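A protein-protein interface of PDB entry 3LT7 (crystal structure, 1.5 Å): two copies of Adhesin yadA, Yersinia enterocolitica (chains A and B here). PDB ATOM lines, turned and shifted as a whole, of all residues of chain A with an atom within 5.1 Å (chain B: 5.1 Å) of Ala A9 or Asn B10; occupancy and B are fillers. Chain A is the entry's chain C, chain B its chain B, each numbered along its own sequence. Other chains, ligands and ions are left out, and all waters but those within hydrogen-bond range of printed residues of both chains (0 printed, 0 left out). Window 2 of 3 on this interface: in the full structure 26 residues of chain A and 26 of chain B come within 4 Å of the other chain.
OD1 of Asp B14 sits at hydrogen-bond distance from OH of Tyr A12.
The side-chain hydroxyl of Thr B13 is in hydrogen-bond range of the side-chain hydroxyl of Thr A13, at 3.3 Å.
O of Ala B9 is in hydrogen-bond range of OG1 of Thr B13 (3.1 Å).
OD1 of Asn B10 lies close to O of Leu B6 (3.3 Å).
The side-chain hydroxyl (OG1) of Thr A13 lies within hydrogen-bond range of the backbone carbonyl oxygen (O) of Ala A9 (3.2 Å).
Thr A5 touches Leu B6.
CD2 of Leu B6 touches CG2 of Thr A8, at 3.3 Å.
Ala A9 touches Leu B6.
Asn B10 touches Ala A9 (ND2 to CA, 3.5 Å).
Tyr A12 touches Asn B10.
Asn B10 touches just these residues of chain A: Ala A9 and Tyr A12.
Of the printed residues of chain B, Tyr A12 touches Asn B10 (3.6 Å) and Asp B14 (2.5 Å).
Printed residues of chain B within 4 Å of Thr A13: Thr B13.
Printed residues of chain A within 4 Å of Leu B6: Thr A5, Thr A8 and Ala A9.
The nearest printed residue of chain B that does not touch Thr A8 is Asn B10 (4.6 Å).
Of the 9 printed residues of chain A, 5 touch a printed residue of chain B.
Hydrophobic or aromatic side chains of chain A that line the printed part of chain B: Ala A9 and Tyr A12.
Among the printed residues, no Asp or Glu carboxylate lies within 4 Å of a Lys or Arg side-chain nitrogen of the other chain.
Thr A5 touches Leu B6, but with the chains exchanged Leu A6 does not touch Thr B5 (7.2 Å).
Thr A8 touches Leu B6, but with the chains exchanged Leu A6 does not touch Thr B8 (10.9 Å).
Tyr A12 touches Asn B10, but with the chains exchanged Asn A10 does not touch Tyr B12 (9.7 Å).
Thr A13 touches its own counterpart, Thr B13.
Of the 7 pairs that touch across the chains among the printed residues, 1 has its exchanged pair printed and touching as well.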
ATOM      1  N   THR A   5       1.717  23.275  27.263  1.00  0.00           N
ATOM      2  CA  THR A   5       1.938  21.900  26.786  1.00  0.00           C
ATOM      3  C   THR A   5       1.462  20.870  27.806  1.00  0.00           C
ATOM      4  O   THR A   5       0.716  19.946  27.463  1.00  0.00           O
ATOM      5  CB  THR A   5       3.425  21.661  26.411  1.00  0.00           C
ATOM      6  OG1 THR A   5       3.677  22.165  25.088  1.00  0.00           O
ATOM      7  CG2 THR A   5       3.800  20.174  26.466  1.00  0.00           C
ATOM      8  N   LEU A   6       1.921  21.042  29.048  1.00  0.00           N
ATOM      9  CA  LEU A   6       1.573  20.182  30.160  1.00  0.00           C
ATOM     10  C   LEU A   6       0.049  20.102  30.284  1.00  0.00           C
ATOM     11  O   LEU A   6      -0.513  19.000  30.455  1.00  0.00           O
ATOM     12  CB  LEU A   6       2.176  20.747  31.448  1.00  0.00           C
ATOM     13  CG  LEU A   6       2.609  19.855  32.623  1.00  0.00           C
ATOM     14  CD1 LEU A   6       2.295  20.566  33.952  1.00  0.00           C
ATOM     15  CD2 LEU A   6       2.016  18.452  32.591  1.00  0.00           C
ATOM     16  N   LYS A   7      -0.617  21.262  30.212  1.00  0.00           N
ATOM     17  CA  LYS A   7      -2.080  21.312  30.238  1.00  0.00           C
ATOM     18  C   LYS A   7      -2.661  20.467  29.099  1.00  0.00           C
ATOM     19  O   LYS A   7      -3.634  19.716  29.318  1.00  0.00           O
ATOM     20  CB  LYS A   7      -2.616  22.761  30.195  1.00  0.00           C
ATOM     21  CG  LYS A   7      -4.144  22.854  30.215  1.00  0.00           C
ATOM     22  CD  LYS A   7      -4.683  24.246  30.591  1.00  0.00           C
ATOM     23  CE  LYS A   7      -6.213  24.322  30.468  1.00  0.00           C
ATOM     24  NZ  LYS A   7      -6.959  23.439  31.440  1.00  0.00           N
ATOM     25  N   THR A   8      -2.055  20.576  27.907  1.00  0.00           N
ATOM     26  CA  THR A   8      -2.473  19.804  26.711  1.00  0.00           C
ATOM     27  C   THR A   8      -2.277  18.271  26.807  1.00  0.00           C
ATOM     28  O   THR A   8      -3.154  17.500  26.367  1.00  0.00           O
ATOM     29  CB  THR A   8      -1.840  20.325  25.372  1.00  0.00           C
ATOM     30  OG1 THR A   8      -1.981  21.751  25.265  1.00  0.00           O
ATOM     31  CG2 THR A   8      -2.509  19.671  24.150  1.00  0.00           C
ATOM     32  N   ALA A   9      -1.138  17.830  27.341  1.00  0.00           N
ATOM     33  CA  ALA A   9      -0.938  16.407  27.633  1.00  0.00           C
ATOM     34  C   ALA A   9      -2.003  15.907  28.625  1.00  0.00           C
ATOM     35  O   ALA A   9      -2.836  15.078  28.256  1.00  0.00           O
ATOM     36  CB  ALA A   9       0.462  16.155  28.147  1.00  0.00           C
ATOM     37  N   ASN A  10      -1.985  16.421  29.865  1.00  0.00           N
ATOM     38  CA  ASN A  10      -2.973  16.063  30.900  1.00  0.00           C
ATOM     39  C   ASN A  10      -4.437  15.988  30.444  1.00  0.00           C
ATOM     40  O   ASN A  10      -5.164  15.059  30.832  1.00  0.00           O
ATOM     41  CB  ASN A  10      -2.887  16.996  32.101  1.00  0.00           C
ATOM     42  CG  ASN A  10      -1.555  16.926  32.809  1.00  0.00           C
ATOM     43  OD1 ASN A  10      -0.814  15.954  32.699  1.00  0.00           O
ATOM     44  ND2 ASN A  10      -1.243  17.969  33.546  1.00  0.00           N
ATOM     45  N   SER A  11      -4.884  16.955  29.641  1.00  0.00           N
ATOM     46  CA  SER A  11      -6.296  16.951  29.234  1.00  0.00           C
ATOM     47  C   SER A  11      -6.571  15.949  28.120  1.00  0.00           C
ATOM     48  O   SER A  11      -7.689  15.442  28.013  1.00  0.00           O
ATOM     49  CB  SER A  11      -6.841  18.354  28.937  1.00  0.00           C
ATOM     50  OG  SER A  11      -6.569  18.746  27.620  1.00  0.00           O
ATOM     51  N   TYR A  12      -5.542  15.623  27.347  1.00  0.00           N
ATOM     52  CA  TYR A  12      -5.591  14.448  26.471  1.00  0.00           C
ATOM     53  C   TYR A  12      -5.734  13.154  27.326  1.00  0.00           C
ATOM     54  O   TYR A  12      -6.649  12.333  27.078  1.00  0.00           O
ATOM     55  CB  TYR A  12      -4.379  14.432  25.522  1.00  0.00           C
ATOM     56  CG  TYR A  12      -4.396  13.351  24.489  1.00  0.00           C
ATOM     57  CD1 TYR A  12      -5.330  13.365  23.445  1.00  0.00           C
ATOM     58  CD2 TYR A  12      -3.477  12.319  24.542  1.00  0.00           C
ATOM     59  CE1 TYR A  12      -5.331  12.382  22.487  1.00  0.00           C
ATOM     60  CE2 TYR A  12      -3.486  11.325  23.618  1.00  0.00           C
ATOM     61  CZ  TYR A  12      -4.414  11.369  22.577  1.00  0.00           C
ATOM     62  OH  TYR A  12      -4.489  10.402  21.625  1.00  0.00           O
ATOM     63  N   THR A  13      -4.863  13.001  28.330  1.00  0.00           N
ATOM     64  CA  THR A  13      -4.967  11.918  29.316  1.00  0.00           C
ATOM     65  C   THR A  13      -6.366  11.763  29.904  1.00  0.00           C
ATOM     66  O   THR A  13      -6.949  10.666  29.821  1.00  0.00           O
ATOM     67  CB  THR A  13      -3.929  12.043  30.429  1.00  0.00           C
ATOM     68  OG1 THR A  13      -2.641  12.351  29.867  1.00  0.00           O
ATOM     69  CG2 THR A  13      -3.852  10.729  31.180  1.00  0.00           C
ATOM     70  N   THR B   5       7.588  17.700  22.667  1.00  0.00           N
ATOM     71  CA  THR B   5       7.208  17.165  23.974  1.00  0.00           C
ATOM     72  C   THR B   5       5.742  16.803  24.063  1.00  0.00           C
ATOM     73  O   THR B   5       5.395  15.854  24.762  1.00  0.00           O
ATOM     74  CB  THR B   5       7.533  18.131  25.096  1.00  0.00           C
ATOM     75  OG1 THR B   5       8.791  18.736  24.822  1.00  0.00           O
ATOM     76  CG2 THR B   5       7.612  17.397  26.429  1.00  0.00           C
ATOM     77  N   LEU B   6       4.877  17.525  23.347  1.00  0.00           N
ATOM     78  CA  LEU B   6       3.465  17.120  23.298  1.00  0.00           C
ATOM     79  C   LEU B   6       3.258  15.826  22.509  1.00  0.00           C
ATOM     80  O   LEU B   6       2.178  15.222  22.617  1.00  0.00           O
ATOM     81  CB  LEU B   6       2.532  18.242  22.786  1.00  0.00           C
ATOM     82  CG  LEU B   6       1.010  18.105  22.957  1.00  0.00           C
ATOM     83  CD1 LEU B   6       0.613  17.876  24.403  1.00  0.00           C
ATOM     84  CD2 LEU B   6       0.310  19.349  22.413  1.00  0.00           C
ATOM     85  N   LYS B   7       4.272  15.403  21.742  1.00  0.00           N
ATOM     86  CA  LYS B   7       4.188  14.186  20.882  1.00  0.00           C
ATOM     87  C   LYS B   7       4.674  12.959  21.649  1.00  0.00           C
ATOM     88  O   LYS B   7       4.056  11.887  21.540  1.00  0.00           O
ATOM     89  CB  LYS B   7       4.964  14.313  19.569  1.00  0.00           C
ATOM     90  CG  LYS B   7       4.361  13.489  18.392  1.00  0.00           C
ATOM     91  CD  LYS B   7       4.529  14.212  17.062  1.00  0.00           C
ATOM     92  CE  LYS B   7       3.647  13.635  15.953  1.00  0.00           C
ATOM     93  NZ  LYS B   7       4.234  12.384  15.375  1.00  0.00           N
ATOM     94  N   THR B   8       5.728  13.116  22.451  1.00  0.00           N
ATOM     95  CA  THR B   8       6.236  11.986  23.250  1.00  0.00           C
ATOM     96  C   THR B   8       5.283  11.669  24.410  1.00  0.00           C
ATOM     97  O   THR B   8       4.922  10.481  24.616  1.00  0.00           O
ATOM     98  CB  THR B   8       7.667  12.175  23.759  1.00  0.00           C
ATOM     99  OG1 THR B   8       8.467  12.805  22.749  1.00  0.00           O
ATOM    100  CG2 THR B   8       8.282  10.805  24.119  1.00  0.00           C
ATOM    101  N   ALA B   9       4.855  12.698  25.149  1.00  0.00           N
ATOM    102  CA  ALA B   9       3.790  12.531  26.171  1.00  0.00           C
ATOM    103  C   ALA B   9       2.448  12.043  25.642  1.00  0.00           C
ATOM    104  O   ALA B   9       1.749  11.315  26.347  1.00  0.00           O
ATOM    105  CB  ALA B   9       3.581  13.807  27.001  1.00  0.00           C
ATOM    106  N   ASN B  10       2.063  12.418  24.421  1.00  0.00           N
ATOM    107  CA  ASN B  10       0.783  11.934  23.895  1.00  0.00           C
ATOM    108  C   ASN B  10       0.772  10.464  23.401  1.00  0.00           C
ATOM    109  O   ASN B  10      -0.226   9.743  23.643  1.00  0.00           O
ATOM    110  CB  ASN B  10       0.123  12.939  22.920  1.00  0.00           C
ATOM    111  CG  ASN B  10      -0.471  14.161  23.638  1.00  0.00           C
ATOM    112  OD1 ASN B  10      -1.103  15.010  23.008  1.00  0.00           O
ATOM    113  ND2 ASN B  10      -0.263  14.252  24.946  1.00  0.00           N
ATOM    114  N   SER B  11       1.876  10.038  22.763  1.00  0.00           N
ATOM    115  CA  SER B  11       2.112   8.639  22.348  1.00  0.00           C
ATOM    116  C   SER B  11       2.316   7.733  23.574  1.00  0.00           C
ATOM    117  O   SER B  11       2.045   6.525  23.562  1.00  0.00           O
ATOM    118  CB  SER B  11       3.349   8.551  21.438  1.00  0.00           C
ATOM    119  OG  SER B  11       3.042   8.912  20.087  1.00  0.00           O
ATOM    120  N   TYR B  12       2.877   8.310  24.624  1.00  0.00           N
ATOM    121  CA  TYR B  12       3.034   7.547  25.848  1.00  0.00           C
ATOM    122  C   TYR B  12       1.611   7.304  26.353  1.00  0.00           C
ATOM    123  O   TYR B  12       1.202   6.149  26.573  1.00  0.00           O
ATOM    124  CB  TYR B  12       3.860   8.297  26.871  1.00  0.00           C
ATOM    125  CG  TYR B  12       4.057   7.525  28.167  1.00  0.00           C
ATOM    126  CD1 TYR B  12       5.001   6.486  28.270  1.00  0.00           C
ATOM    127  CD2 TYR B  12       3.294   7.826  29.280  1.00  0.00           C
ATOM    128  CE1 TYR B  12       5.166   5.799  29.490  1.00  0.00           C
ATOM    129  CE2 TYR B  12       3.454   7.169  30.500  1.00  0.00           C
ATOM    130  CZ  TYR B  12       4.378   6.156  30.605  1.00  0.00           C
ATOM    131  OH  TYR B  12       4.495   5.533  31.833  1.00  0.00           O
ATOM    132  N   THR B  13       0.834   8.378  26.474  1.00  0.00           N
ATOM    133  CA  THR B  13      -0.564   8.247  26.921  1.00  0.00           C
ATOM    134  C   THR B  13      -1.419   7.274  26.092  1.00  0.00           C
ATOM    135  O   THR B  13      -2.300   6.613  26.657  1.00  0.00           O
ATOM    136  CB  THR B  13      -1.356   9.600  26.995  1.00  0.00           C
ATOM    137  OG1 THR B  13      -0.717  10.432  27.959  1.00  0.00           O
ATOM    138  CG2 THR B  13      -2.852   9.399  27.301  1.00  0.00           C
ATOM    139  N   ASP B  14      -1.223   7.235  24.759  1.00  0.00           N
ATOM    140  CA  ASP B  14      -2.005   6.324  23.943  1.00  0.00           C
ATOM    141  C   ASP B  14      -1.608   4.864  24.170  1.00  0.00           C
ATOM    142  O   ASP B  14      -2.480   4.009  24.204  1.00  0.00           O
ATOM    143  CB  ASP B  14      -1.896   6.614  22.443  1.00  0.00           C
ATOM    144  CG  ASP B  14      -2.230   8.029  22.100  1.00  0.00           C
ATOM    145  OD1 ASP B  14      -3.135   8.597  22.746  1.00  0.00           O
ATOM    146  OD2 ASP B  14      -1.644   8.561  21.136  1.00  0.00           O
